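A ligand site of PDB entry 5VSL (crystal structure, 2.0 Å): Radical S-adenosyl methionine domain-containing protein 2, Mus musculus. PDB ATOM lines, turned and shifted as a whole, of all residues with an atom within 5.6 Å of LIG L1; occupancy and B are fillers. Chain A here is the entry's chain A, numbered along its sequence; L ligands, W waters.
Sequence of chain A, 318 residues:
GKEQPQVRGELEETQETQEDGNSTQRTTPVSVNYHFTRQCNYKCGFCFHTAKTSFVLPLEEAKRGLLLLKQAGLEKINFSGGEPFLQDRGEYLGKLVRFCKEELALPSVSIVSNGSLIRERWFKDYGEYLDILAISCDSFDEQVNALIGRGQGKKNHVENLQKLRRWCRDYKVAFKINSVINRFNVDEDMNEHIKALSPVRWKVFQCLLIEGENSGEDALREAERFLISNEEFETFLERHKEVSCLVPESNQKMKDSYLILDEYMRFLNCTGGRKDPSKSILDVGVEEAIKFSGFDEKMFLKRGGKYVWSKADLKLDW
An oxygen (O2) of LIG L1 lies within hydrogen-bond range of the side-chain hydroxyl (OG) of Ser 136.
The backbone carbonyl oxygen (O) of Gly 82 lies close to a nitrogen (N1) of LIG L1 (2.6 Å).
N5 of LIG L1 lies within hydrogen-bond range of N of Leu 208 (2.9 Å).
A nitrogen (N4) of LIG L1 lies within hydrogen-bond range of the backbone carbonyl oxygen (O) of Leu 208 (3.0 Å).
O of Phe 46 is in hydrogen-bond range of N4 of LIG L1 (2.9 Å).
N of Ser 113 sits close to O2 of LIG L1 (3.4 Å).
An oxygen (O2) of LIG L1 sits close to the backbone carbonyl oxygen of Ser 113 (3.0 Å).
The guanidinium group (NH2) of Arg 150 lies within hydrogen-bond range of an oxygen (O5) of LIG L1, 3.0 Å away.
N3 of LIG L1 lies within hydrogen-bond range of N of Phe 48 (3.2 Å).
An oxygen (O2) of LIG L1 lies within hydrogen-bond range of the backbone NH (N) of Asn 114 (3.2 Å).
ND2 of Asn 178 sits at hydrogen-bond distance from O4 of LIG L1.
N1 of LIG L1 lies close to OE1 of Glu 83 (3.4 Å).
A nitrogen (N4) of LIG L1 sits close to the side-chain amide nitrogen (ND2) of Asn 214, 3.4 Å away.
The backbone NH (N) of Gly 82 sits close to a sulfur (S2) of LG2 L2 (3.5 Å).
A sulfur (S3) of LG2 L2 lies close to the guanidinium group (NH1) of Arg 150 (3.3 Å).
ND2 of Asn 114 sits close to S3 of LG2 L2.
The side-chain sulfur (SG) of Cys 47 binds an iron atom (FE3) of LG2 L2 (2.5 Å).
The side-chain sulfur of Cys 40 binds an iron atom (FE1) of LG2 L2, at 2.4 Å.
FE4 of LG2 L2 is bound by O1 of LIG L1, 2.4 Å away.
The backbone carbonyl oxygen (O) of Ser 113 lies within hydrogen-bond range of the backbone NH (N) of Ser 136.
The side-chain amide nitrogen (ND2) of Asn 214 sits at hydrogen-bond distance from the backbone carbonyl oxygen (O) of Phe 46, 2.9 Å away.
The side-chain hydroxyl (OG) of Ser 113 lies within hydrogen-bond range of the side-chain carboxylate (OE2) of Glu 83, at 2.7 Å.
The side-chain carboxylate of Asp 138 lies within salt-bridge range of the guanidinium group of Arg 150 (2.8 Å).
OE1 of Glu 83 sits at hydrogen-bond distance from N of Asn 114, at 2.8 Å.
The side-chain carboxylate of Asp 138 is in hydrogen-bond range of the backbone NH of Val 180.
The backbone carbonyl oxygen of Asn 214 lies within hydrogen-bond range of the backbone NH of Ala 223.
The backbone carbonyl oxygen (O) of Gly 81 sits at hydrogen-bond distance from a ring nitrogen (ND1) of His 35 (2.7 Å).
Merely in contact with LIG L1: Cys 47, Ser 80, Gly 81, Val 112, Val 180, Phe 205, Gln 206 and Cys 207.
Hydrophobic or aromatic side chains that line LIG L1: Phe 46, Phe 48, Val 112, Val 180, Phe 205 and Leu 208.
Within 4 Å of LIG L1: Phe 46, Cys 47, Phe 48, Ser 80, Gly 81, Gly 82, Glu 83, Val 112, Ser 113, Asn 114, Ser 136, Arg 150, Asn 178, Val 180, Phe 205, Gln 206, Cys 207, Leu 208 and Asn 214.
Along chain A the residues within 4 Å of LIG L1 span positions 46 to 214.
The nearest printed residue that does not touch LIG L1 is Pro 84 (4.2 Å).
Water W2 lies within hydrogen-bond range of O5 of LIG L1 (2.7 Å), OD1 of Asp 138 (2.8 Å), NH2 of Arg 150 (3.1 Å), O of Asn 178 (3.2 Å) and OG of Ser 136 (3.3 Å).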
ATOM      1  N   HIS A  35     -17.235  -2.378 -27.787  1.00  0.00           N
ATOM      2  CA  HIS A  35     -17.598  -1.992 -26.421  1.00  0.00           C
ATOM      3  C   HIS A  35     -17.900  -0.503 -26.418  1.00  0.00           C
ATOM      4  O   HIS A  35     -17.076   0.346 -26.058  1.00  0.00           O
ATOM      5  CB  HIS A  35     -16.472  -2.345 -25.448  1.00  0.00           C
ATOM      6  CG  HIS A  35     -16.244  -3.824 -25.295  1.00  0.00           C
ATOM      7  ND1 HIS A  35     -16.508  -4.495 -24.122  1.00  0.00           N
ATOM      8  CD2 HIS A  35     -15.793  -4.744 -26.173  1.00  0.00           C
ATOM      9  CE1 HIS A  35     -16.211  -5.778 -24.282  1.00  0.00           C
ATOM     10  NE2 HIS A  35     -15.774  -5.949 -25.515  1.00  0.00           N
ATOM     11  N   CYS A  40     -22.257   0.675 -16.469  1.00  0.00           N
ATOM     12  CA  CYS A  40     -22.946  -0.571 -16.152  1.00  0.00           C
ATOM     13  C   CYS A  40     -23.696  -0.413 -14.830  1.00  0.00           C
ATOM     14  O   CYS A  40     -23.343   0.408 -13.995  1.00  0.00           O
ATOM     15  CB  CYS A  40     -21.982  -1.748 -16.072  1.00  0.00           C
ATOM     16  SG  CYS A  40     -22.864  -3.292 -15.884  1.00  0.00           S
ATOM     17  N   PHE A  46     -14.809  -9.176 -10.961  1.00  0.00           N
ATOM     18  CA  PHE A  46     -13.755  -9.508 -11.923  1.00  0.00           C
ATOM     19  C   PHE A  46     -13.836  -8.715 -13.223  1.00  0.00           C
ATOM     20  O   PHE A  46     -12.993  -8.924 -14.106  1.00  0.00           O
ATOM     21  CB  PHE A  46     -13.774 -11.014 -12.238  1.00  0.00           C
ATOM     22  CG  PHE A  46     -15.130 -11.506 -12.720  1.00  0.00           C
ATOM     23  CD1 PHE A  46     -15.628 -11.129 -13.960  1.00  0.00           C
ATOM     24  CD2 PHE A  46     -15.899 -12.331 -11.917  1.00  0.00           C
ATOM     25  CE1 PHE A  46     -16.882 -11.563 -14.387  1.00  0.00           C
ATOM     26  CE2 PHE A  46     -17.139 -12.780 -12.343  1.00  0.00           C
ATOM     27  CZ  PHE A  46     -17.628 -12.393 -13.581  1.00  0.00           C
ATOM     28  N   CYS A  47     -14.822  -7.836 -13.356  1.00  0.00           N
ATOM     29  CA  CYS A  47     -15.081  -7.126 -14.608  1.00  0.00           C
ATOM     30  C   CYS A  47     -13.801  -6.622 -15.261  1.00  0.00           C
ATOM     31  O   CYS A  47     -13.030  -5.888 -14.652  1.00  0.00           O
ATOM     32  CB  CYS A  47     -16.020  -5.960 -14.348  1.00  0.00           C
ATOM     33  SG  CYS A  47     -16.281  -4.990 -15.825  1.00  0.00           S
ATOM     34  N   PHE A  48     -13.545  -7.048 -16.502  1.00  0.00           N
ATOM     35  CA  PHE A  48     -12.309  -6.669 -17.178  1.00  0.00           C
ATOM     36  C   PHE A  48     -12.499  -5.520 -18.166  1.00  0.00           C
ATOM     37  O   PHE A  48     -11.578  -5.196 -18.927  1.00  0.00           O
ATOM     38  CB  PHE A  48     -11.675  -7.886 -17.865  1.00  0.00           C
ATOM     39  CG  PHE A  48     -12.376  -8.360 -19.132  1.00  0.00           C
ATOM     40  CD1 PHE A  48     -11.732  -9.249 -19.987  1.00  0.00           C
ATOM     41  CD2 PHE A  48     -13.651  -7.917 -19.483  1.00  0.00           C
ATOM     42  CE1 PHE A  48     -12.359  -9.688 -21.148  1.00  0.00           C
ATOM     43  CE2 PHE A  48     -14.275  -8.339 -20.642  1.00  0.00           C
ATOM     44  CZ  PHE A  48     -13.616  -9.227 -21.480  1.00  0.00           C
ATOM     45  N   HIS A  49     -13.663  -4.869 -18.163  1.00  0.00           N
ATOM     46  CA  HIS A  49     -13.908  -3.695 -19.013  1.00  0.00           C
ATOM     47  C   HIS A  49     -14.700  -2.673 -18.191  1.00  0.00           C
ATOM     48  O   HIS A  49     -15.919  -2.563 -18.343  1.00  0.00           O
ATOM     49  CB  HIS A  49     -14.613  -4.051 -20.315  1.00  0.00           C
ATOM     50  CG  HIS A  49     -14.417  -3.012 -21.378  1.00  0.00           C
ATOM     51  ND1 HIS A  49     -13.241  -2.884 -22.088  1.00  0.00           N
ATOM     52  CD2 HIS A  49     -15.224  -2.009 -21.791  1.00  0.00           C
ATOM     53  CE1 HIS A  49     -13.340  -1.859 -22.907  1.00  0.00           C
ATOM     54  NE2 HIS A  49     -14.535  -1.311 -22.758  1.00  0.00           N
ATOM     55  N   SER A  80     -21.098  -4.709 -27.017  1.00  0.00           N
ATOM     56  CA  SER A  80     -20.748  -5.082 -25.655  1.00  0.00           C
ATOM     57  C   SER A  80     -20.446  -3.803 -24.865  1.00  0.00           C
ATOM     58  O   SER A  80     -20.748  -2.699 -25.313  1.00  0.00           O
ATOM     59  CB  SER A  80     -19.573  -6.066 -25.660  1.00  0.00           C
ATOM     60  OG  SER A  80     -19.414  -6.705 -24.395  1.00  0.00           O
ATOM     61  N   GLY A  81     -19.868  -3.971 -23.677  1.00  0.00           N
ATOM     62  CA  GLY A  81     -19.529  -2.833 -22.842  1.00  0.00           C
ATOM     63  C   GLY A  81     -18.710  -3.212 -21.614  1.00  0.00           C
ATOM     64  O   GLY A  81     -17.767  -4.009 -21.738  1.00  0.00           O
ATOM     65  N   GLY A  82     -19.056  -2.710 -20.430  1.00  0.00           N
ATOM     66  CA  GLY A  82     -20.251  -1.910 -20.205  1.00  0.00           C
ATOM     67  C   GLY A  82     -21.534  -2.724 -20.328  1.00  0.00           C
ATOM     68  O   GLY A  82     -21.483  -3.881 -20.729  1.00  0.00           O
ATOM     69  N   GLU A  83     -22.684  -2.137 -20.013  1.00  0.00           N
ATOM     70  CA  GLU A  83     -23.950  -2.819 -20.252  1.00  0.00           C
ATOM     71  C   GLU A  83     -24.639  -2.179 -21.449  1.00  0.00           C
ATOM     72  O   GLU A  83     -25.091  -1.019 -21.356  1.00  0.00           O
ATOM     73  CB  GLU A  83     -24.851  -2.752 -19.015  1.00  0.00           C
ATOM     74  CG  GLU A  83     -26.261  -3.281 -19.264  1.00  0.00           C
ATOM     75  CD  GLU A  83     -26.285  -4.599 -20.024  1.00  0.00           C
ATOM     76  OE1 GLU A  83     -25.519  -5.534 -19.676  1.00  0.00           O
ATOM     77  OE2 GLU A  83     -27.079  -4.702 -20.983  1.00  0.00           O
ATOM     78  N   PRO A  84     -24.734  -2.885 -22.575  1.00  0.00           N
ATOM     79  CA  PRO A  84     -25.262  -2.260 -23.808  1.00  0.00           C
ATOM     80  C   PRO A  84     -26.661  -1.700 -23.688  1.00  0.00           C
ATOM     81  O   PRO A  84     -26.977  -0.706 -24.368  1.00  0.00           O
ATOM     82  CB  PRO A  84     -25.195  -3.412 -24.815  1.00  0.00           C
ATOM     83  CG  PRO A  84     -24.055  -4.221 -24.325  1.00  0.00           C
ATOM     84  CD  PRO A  84     -24.195  -4.221 -22.841  1.00  0.00           C
ATOM     85  N   VAL A 112     -23.966  -8.785 -26.277  1.00  0.00           N
ATOM     86  CA  VAL A 112     -23.668  -9.446 -25.008  1.00  0.00           C
ATOM     87  C   VAL A 112     -24.199  -8.558 -23.887  1.00  0.00           C
ATOM     88  O   VAL A 112     -23.819  -7.387 -23.810  1.00  0.00           O
ATOM     89  CB  VAL A 112     -22.153  -9.700 -24.817  1.00  0.00           C
ATOM     90  CG1 VAL A 112     -21.898 -10.539 -23.568  1.00  0.00           C
ATOM     91  CG2 VAL A 112     -21.537 -10.363 -26.038  1.00  0.00           C
ATOM     92  N   SER A 113     -25.040  -9.104 -23.023  1.00  0.00           N
ATOM     93  CA  SER A 113     -25.730  -8.291 -22.031  1.00  0.00           C
ATOM     94  C   SER A 113     -25.790  -9.036 -20.698  1.00  0.00           C
ATOM     95  O   SER A 113     -25.846 -10.268 -20.683  1.00  0.00           O
ATOM     96  CB  SER A 113     -27.166  -7.952 -22.505  1.00  0.00           C
ATOM     97  OG  SER A 113     -27.884  -7.208 -21.536  1.00  0.00           O
ATOM     98  N   ASN A 114     -25.814  -8.277 -19.578  1.00  0.00           N
ATOM     99  CA  ASN A 114     -26.160  -8.924 -18.314  1.00  0.00           C
ATOM    100  C   ASN A 114     -27.663  -9.216 -18.208  1.00  0.00           C
ATOM    101  O   ASN A 114     -28.076  -9.889 -17.257  1.00  0.00           O
ATOM    102  CB  ASN A 114     -25.653  -8.113 -17.093  1.00  0.00           C
ATOM    103  CG  ASN A 114     -26.395  -6.778 -16.885  1.00  0.00           C
ATOM    104  OD1 ASN A 114     -27.565  -6.632 -17.192  1.00  0.00           O
ATOM    105  ND2 ASN A 114     -25.687  -5.804 -16.310  1.00  0.00           N
ATOM    106  N   ALA A 134     -26.528 -12.830 -26.364  1.00  0.00           N
ATOM    107  CA  ALA A 134     -25.765 -13.621 -25.397  1.00  0.00           C
ATOM    108  C   ALA A 134     -25.933 -12.996 -24.021  1.00  0.00           C
ATOM    109  O   ALA A 134     -25.665 -11.813 -23.844  1.00  0.00           O
ATOM    110  CB  ALA A 134     -24.282 -13.693 -25.770  1.00  0.00           C
ATOM    111  N   ILE A 135     -26.390 -13.792 -23.056  1.00  0.00           N
ATOM    112  CA  ILE A 135     -26.656 -13.316 -21.713  1.00  0.00           C
ATOM    113  C   ILE A 135     -25.560 -13.865 -20.794  1.00  0.00           C
ATOM    114  O   ILE A 135     -25.305 -15.067 -20.789  1.00  0.00           O
ATOM    115  CB  ILE A 135     -28.068 -13.747 -21.231  1.00  0.00           C
ATOM    116  CG1 ILE A 135     -29.160 -13.209 -22.171  1.00  0.00           C
ATOM    117  CG2 ILE A 135     -28.350 -13.185 -19.826  1.00  0.00           C
ATOM    118  CD1 ILE A 135     -29.138 -11.699 -22.292  1.00  0.00           C
ATOM    119  N   SER A 136     -24.920 -12.985 -20.035  1.00  0.00           N
ATOM    120  CA  SER A 136     -23.894 -13.433 -19.098  1.00  0.00           C
ATOM    121  C   SER A 136     -24.556 -14.078 -17.887  1.00  0.00           C
ATOM    122  O   SER A 136     -25.381 -13.467 -17.215  1.00  0.00           O
ATOM    123  CB  SER A 136     -23.016 -12.266 -18.649  1.00  0.00           C
ATOM    124  OG  SER A 136     -22.313 -11.785 -19.780  1.00  0.00           O
ATOM    125  N   ASP A 138     -22.937 -16.557 -14.752  1.00  0.00           N
ATOM    126  CA  ASP A 138     -21.734 -17.224 -14.270  1.00  0.00           C
ATOM    127  C   ASP A 138     -22.025 -18.359 -13.308  1.00  0.00           C
ATOM    128  O   ASP A 138     -21.136 -19.169 -13.026  1.00  0.00           O
ATOM    129  CB  ASP A 138     -20.810 -16.206 -13.604  1.00  0.00           C
ATOM    130  CG  ASP A 138     -20.469 -15.036 -14.536  1.00  0.00           C
ATOM    131  OD1 ASP A 138     -20.074 -15.285 -15.693  1.00  0.00           O
ATOM    132  OD2 ASP A 138     -20.625 -13.880 -14.107  1.00  0.00           O
ATOM    133  N   ARG A 150     -22.854 -10.103  -9.454  1.00  0.00           N
ATOM    134  CA  ARG A 150     -23.668 -10.213 -10.661  1.00  0.00           C
ATOM    135  C   ARG A 150     -25.128 -10.035 -10.255  1.00  0.00           C
ATOM    136  O   ARG A 150     -25.891 -11.003 -10.100  1.00  0.00           O
ATOM    137  CB  ARG A 150     -23.404 -11.558 -11.353  1.00  0.00           C
ATOM    138  CG  ARG A 150     -24.174 -11.768 -12.640  1.00  0.00           C
ATOM    139  CD  ARG A 150     -23.588 -11.001 -13.802  1.00  0.00           C
ATOM    140  NE  ARG A 150     -22.382 -11.617 -14.341  1.00  0.00           N
ATOM    141  CZ  ARG A 150     -21.812 -11.218 -15.462  1.00  0.00           C
ATOM    142  NH1 ARG A 150     -22.340 -10.202 -16.121  1.00  0.00           N
ATOM    143  NH2 ARG A 150     -20.705 -11.799 -15.919  1.00  0.00           N
ATOM    144  N   ASN A 178     -23.030 -16.665 -21.914  1.00  0.00           N
ATOM    145  CA  ASN A 178     -21.629 -16.388 -21.614  1.00  0.00           C
ATOM    146  C   ASN A 178     -21.400 -16.632 -20.124  1.00  0.00           C
ATOM    147  O   ASN A 178     -22.192 -16.160 -19.307  1.00  0.00           O
ATOM    148  CB  ASN A 178     -21.259 -14.936 -21.954  1.00  0.00           C
ATOM    149  CG  ASN A 178     -20.987 -14.688 -23.451  1.00  0.00           C
ATOM    150  OD1 ASN A 178     -21.287 -15.504 -24.328  1.00  0.00           O
ATOM    151  ND2 ASN A 178     -20.370 -13.549 -23.737  1.00  0.00           N
ATOM    152  N   SER A 179     -20.338 -17.358 -19.775  1.00  0.00           N
ATOM    153  CA  SER A 179     -19.962 -17.608 -18.393  1.00  0.00           C
ATOM    154  C   SER A 179     -18.475 -17.354 -18.211  1.00  0.00           C
ATOM    155  O   SER A 179     -17.650 -17.861 -18.975  1.00  0.00           O
ATOM    156  CB  SER A 179     -20.263 -19.059 -17.963  1.00  0.00           C
ATOM    157  OG  SER A 179     -21.656 -19.316 -18.067  1.00  0.00           O
ATOM    158  N   VAL A 180     -18.140 -16.592 -17.161  1.00  0.00           N
ATOM    159  CA  VAL A 180     -16.761 -16.370 -16.746  1.00  0.00           C
ATOM    160  C   VAL A 180     -16.433 -17.383 -15.664  1.00  0.00           C
ATOM    161  O   VAL A 180     -17.051 -17.378 -14.599  1.00  0.00           O
ATOM    162  CB  VAL A 180     -16.548 -14.932 -16.243  1.00  0.00           C
ATOM    163  CG1 VAL A 180     -15.113 -14.748 -15.737  1.00  0.00           C
ATOM    164  CG2 VAL A 180     -16.856 -13.942 -17.360  1.00  0.00           C
ATOM    165  N   PHE A 205     -15.509 -18.531 -20.602  1.00  0.00           N
ATOM    166  CA  PHE A 205     -14.300 -17.723 -20.562  1.00  0.00           C
ATOM    167  C   PHE A 205     -13.543 -17.991 -19.263  1.00  0.00           C
ATOM    168  O   PHE A 205     -14.125 -17.881 -18.185  1.00  0.00           O
ATOM    169  CB  PHE A 205     -14.619 -16.229 -20.640  1.00  0.00           C
ATOM    170  CG  PHE A 205     -15.377 -15.807 -21.885  1.00  0.00           C
ATOM    171  CD1 PHE A 205     -14.703 -15.225 -22.955  1.00  0.00           C
ATOM    172  CD2 PHE A 205     -16.753 -15.951 -21.971  1.00  0.00           C
ATOM    173  CE1 PHE A 205     -15.404 -14.813 -24.100  1.00  0.00           C
ATOM    174  CE2 PHE A 205     -17.447 -15.545 -23.115  1.00  0.00           C
ATOM    175  CZ  PHE A 205     -16.769 -14.972 -24.171  1.00  0.00           C
ATOM    176  N   GLN A 206     -12.261 -18.304 -19.381  1.00  0.00           N
ATOM    177  CA  GLN A 206     -11.408 -18.283 -18.198  1.00  0.00           C
ATOM    178  C   GLN A 206     -11.268 -16.846 -17.720  1.00  0.00           C
ATOM    179  O   GLN A 206     -11.012 -15.940 -18.518  1.00  0.00           O
ATOM    180  CB  GLN A 206     -10.046 -18.877 -18.505  1.00  0.00           C
ATOM    181  CG  GLN A 206      -9.100 -19.000 -17.304  1.00  0.00           C
ATOM    182  CD  GLN A 206      -7.730 -19.512 -17.733  1.00  0.00           C
ATOM    183  OE1 GLN A 206      -7.447 -19.605 -18.917  1.00  0.00           O
ATOM    184  NE2 GLN A 206      -6.883 -19.852 -16.763  1.00  0.00           N
ATOM    185  N   CYS A 207     -11.465 -16.610 -16.420  1.00  0.00           N
ATOM    186  CA  CYS A 207     -11.294 -15.262 -15.873  1.00  0.00           C
ATOM    187  C   CYS A 207      -9.965 -14.659 -16.318  1.00  0.00           C
ATOM    188  O   CYS A 207      -8.910 -15.265 -16.154  1.00  0.00           O
ATOM    189  CB  CYS A 207     -11.372 -15.297 -14.339  1.00  0.00           C
ATOM    190  SG  CYS A 207     -11.532 -13.633 -13.608  1.00  0.00           S
ATOM    191  N   LEU A 208     -10.032 -13.468 -16.919  1.00  0.00           N
ATOM    192  CA  LEU A 208      -8.873 -12.815 -17.528  1.00  0.00           C
ATOM    193  C   LEU A 208      -8.477 -11.571 -16.742  1.00  0.00           C
ATOM    194  O   LEU A 208      -9.320 -10.724 -16.434  1.00  0.00           O
ATOM    195  CB  LEU A 208      -9.172 -12.442 -18.990  1.00  0.00           C
ATOM    196  CG  LEU A 208      -8.040 -11.899 -19.862  1.00  0.00           C
ATOM    197  CD1 LEU A 208      -6.947 -12.928 -20.025  1.00  0.00           C
ATOM    198  CD2 LEU A 208      -8.587 -11.506 -21.222  1.00  0.00           C
ATOM    199  N   LEU A 209      -7.186 -11.452 -16.426  1.00  0.00           N
ATOM    200  CA  LEU A 209      -6.651 -10.253 -15.809  1.00  0.00           C
ATOM    201  C   LEU A 209      -6.118  -9.324 -16.896  1.00  0.00           C
ATOM    202  O   LEU A 209      -5.332  -9.750 -17.746  1.00  0.00           O
ATOM    203  CB  LEU A 209      -5.519 -10.601 -14.842  1.00  0.00           C
ATOM    204  CG  LEU A 209      -5.192  -9.635 -13.699  1.00  0.00           C
ATOM    205  CD1 LEU A 209      -6.318  -9.643 -12.693  1.00  0.00           C
ATOM    206  CD2 LEU A 209      -3.851 -10.010 -13.033  1.00  0.00           C
ATOM    207  N   ASN A 214      -8.881  -4.573 -14.404  1.00  0.00           N
ATOM    208  CA  ASN A 214      -9.201  -5.265 -13.154  1.00  0.00           C
ATOM    209  C   ASN A 214      -7.927  -5.658 -12.421  1.00  0.00           C
ATOM    210  O   ASN A 214      -7.901  -6.663 -11.725  1.00  0.00           O
ATOM    211  CB  ASN A 214     -10.077  -6.487 -13.414  1.00  0.00           C
ATOM    212  CG  ASN A 214      -9.450  -7.429 -14.418  1.00  0.00           C
ATOM    213  OD1 ASN A 214      -8.299  -7.238 -14.826  1.00  0.00           O
ATOM    214  ND2 ASN A 214     -10.207  -8.426 -14.844  1.00  0.00           N
ATOM    215  N   ALA A 223      -9.129  -8.213  -9.660  1.00  0.00           N
ATOM    216  CA  ALA A 223      -9.646  -9.541  -9.969  1.00  0.00           C
ATOM    217  C   ALA A 223      -8.700 -10.662  -9.587  1.00  0.00           C
ATOM    218  O   ALA A 223      -9.034 -11.827  -9.814  1.00  0.00           O
ATOM    219  CB  ALA A 223      -9.965  -9.628 -11.460  1.00  0.00           C
ATOM    220  N   MET A 254      -8.240 -15.584 -25.708  1.00  0.00           N
ATOM    221  CA  MET A 254      -8.692 -14.191 -25.641  1.00  0.00           C
ATOM    222  C   MET A 254      -7.567 -13.226 -26.003  1.00  0.00           C
ATOM    223  O   MET A 254      -7.789 -12.241 -26.713  1.00  0.00           O
ATOM    224  CB  MET A 254      -9.237 -13.878 -24.256  1.00  0.00           C
ATOM    225  CG  MET A 254     -10.545 -14.594 -23.960  1.00  0.00           C
ATOM    226  SD  MET A 254     -11.893 -13.916 -24.969  1.00  0.00           S
ATOM    227  CE  MET A 254     -12.169 -12.403 -24.037  1.00  0.00           C
ATOM    228  N   TYR A 258      -9.315 -11.936 -29.295  1.00  0.00           N
ATOM    229  CA  TYR A 258     -10.399 -11.060 -28.869  1.00  0.00           C
ATOM    230  C   TYR A 258      -9.959  -9.616 -29.079  1.00  0.00           C
ATOM    231  O   TYR A 258      -9.119  -9.098 -28.340  1.00  0.00           O
ATOM    232  CB  TYR A 258     -10.792 -11.327 -27.413  1.00  0.00           C
ATOM    233  CG  TYR A 258     -12.108 -10.673 -27.037  1.00  0.00           C
ATOM    234  CD1 TYR A 258     -13.317 -11.337 -27.203  1.00  0.00           C
ATOM    235  CD2 TYR A 258     -12.143  -9.373 -26.559  1.00  0.00           C
ATOM    236  CE1 TYR A 258     -14.516 -10.741 -26.879  1.00  0.00           C
ATOM    237  CE2 TYR A 258     -13.337  -8.759 -26.248  1.00  0.00           C
ATOM    238  CZ  TYR A 258     -14.528  -9.447 -26.398  1.00  0.00           C
ATOM    239  OH  TYR A 258     -15.710  -8.820 -26.062  1.00  0.00           O
HETATM  240  N1  LIG L   1     -22.182  -6.126 -19.528  1.00  0.00           N
HETATM  241  C1  LIG L   1     -22.406  -7.232 -20.487  1.00  0.00           C
HETATM  242  C2  LIG L   1     -21.327  -7.260 -21.573  1.00  0.00           C
HETATM  243  C3  LIG L   1     -20.025  -6.561 -21.163  1.00  0.00           C
HETATM  244  S1  LIG L   1     -18.878  -7.694 -20.467  1.00  0.00           S
HETATM  245  C4  LIG L   1     -22.461  -8.559 -19.777  1.00  0.00           C
HETATM  246  O1  LIG L   1     -22.054  -8.726 -18.628  1.00  0.00           O
HETATM  247  O2  LIG L   1     -22.934  -9.532 -20.347  1.00  0.00           O
HETATM  248  C5  LIG L   1     -18.566  -8.657 -21.933  1.00  0.00           C
HETATM  249  C6  LIG L   1     -18.288 -10.134 -21.609  1.00  0.00           C
HETATM  250  O3  LIG L   1     -16.993 -10.227 -21.008  1.00  0.00           O
HETATM  251  C7  LIG L   1     -19.294 -10.730 -20.623  1.00  0.00           C
HETATM  252  O4  LIG L   1     -19.667 -12.101 -20.907  1.00  0.00           O
HETATM  253  C8  LIG L   1     -18.496 -10.714 -19.347  1.00  0.00           C
HETATM  254  O5  LIG L   1     -19.035 -11.586 -18.350  1.00  0.00           O
HETATM  255  C9  LIG L   1     -17.120 -11.062 -19.891  1.00  0.00           C
HETATM  256  N2  LIG L   1     -16.093 -10.750 -18.876  1.00  0.00           N
HETATM  257  C10 LIG L   1     -16.144  -9.756 -17.979  1.00  0.00           C
HETATM  258  N3  LIG L   1     -15.050  -9.778 -17.179  1.00  0.00           N
HETATM  259  C11 LIG L   1     -14.291 -10.806 -17.583  1.00  0.00           C
HETATM  260  C12 LIG L   1     -12.995 -11.377 -17.175  1.00  0.00           C
HETATM  261  N4  LIG L   1     -12.310 -10.836 -16.134  1.00  0.00           N
HETATM  262  N5  LIG L   1     -12.534 -12.454 -17.862  1.00  0.00           N
HETATM  263  C13 LIG L   1     -13.227 -12.989 -18.889  1.00  0.00           C
HETATM  264  N6  LIG L   1     -14.400 -12.510 -19.323  1.00  0.00           N
HETATM  265  C14 LIG L   1     -14.966 -11.440 -18.715  1.00  0.00           C
HETATM  266 FE1  LG2 L   2     -21.110  -4.903 -15.945  1.00  0.00          FE
HETATM  267 FE2  LG2 L   2     -20.422  -7.281 -14.863  1.00  0.00          FE
HETATM  268 FE3  LG2 L   2     -18.616  -5.808 -16.049  1.00  0.00          FE
HETATM  269 FE4  LG2 L   2     -20.769  -6.948 -17.581  1.00  0.00          FE
HETATM  270  S1  LG2 L   2     -18.909  -7.927 -16.334  1.00  0.00           S
HETATM  271  S2  LG2 L   2     -19.708  -4.706 -17.649  1.00  0.00           S
HETATM  272  S3  LG2 L   2     -22.376  -6.866 -16.022  1.00  0.00           S
HETATM  273  S4  LG2 L   2     -19.697  -5.156 -14.128  1.00  0.00           S
HETATM  274  O   HOH W   1     -15.708 -11.766 -23.029  1.00  0.00           O
HETATM  275  O   HOH W   2     -20.322 -13.894 -18.133  1.00  0.00           O
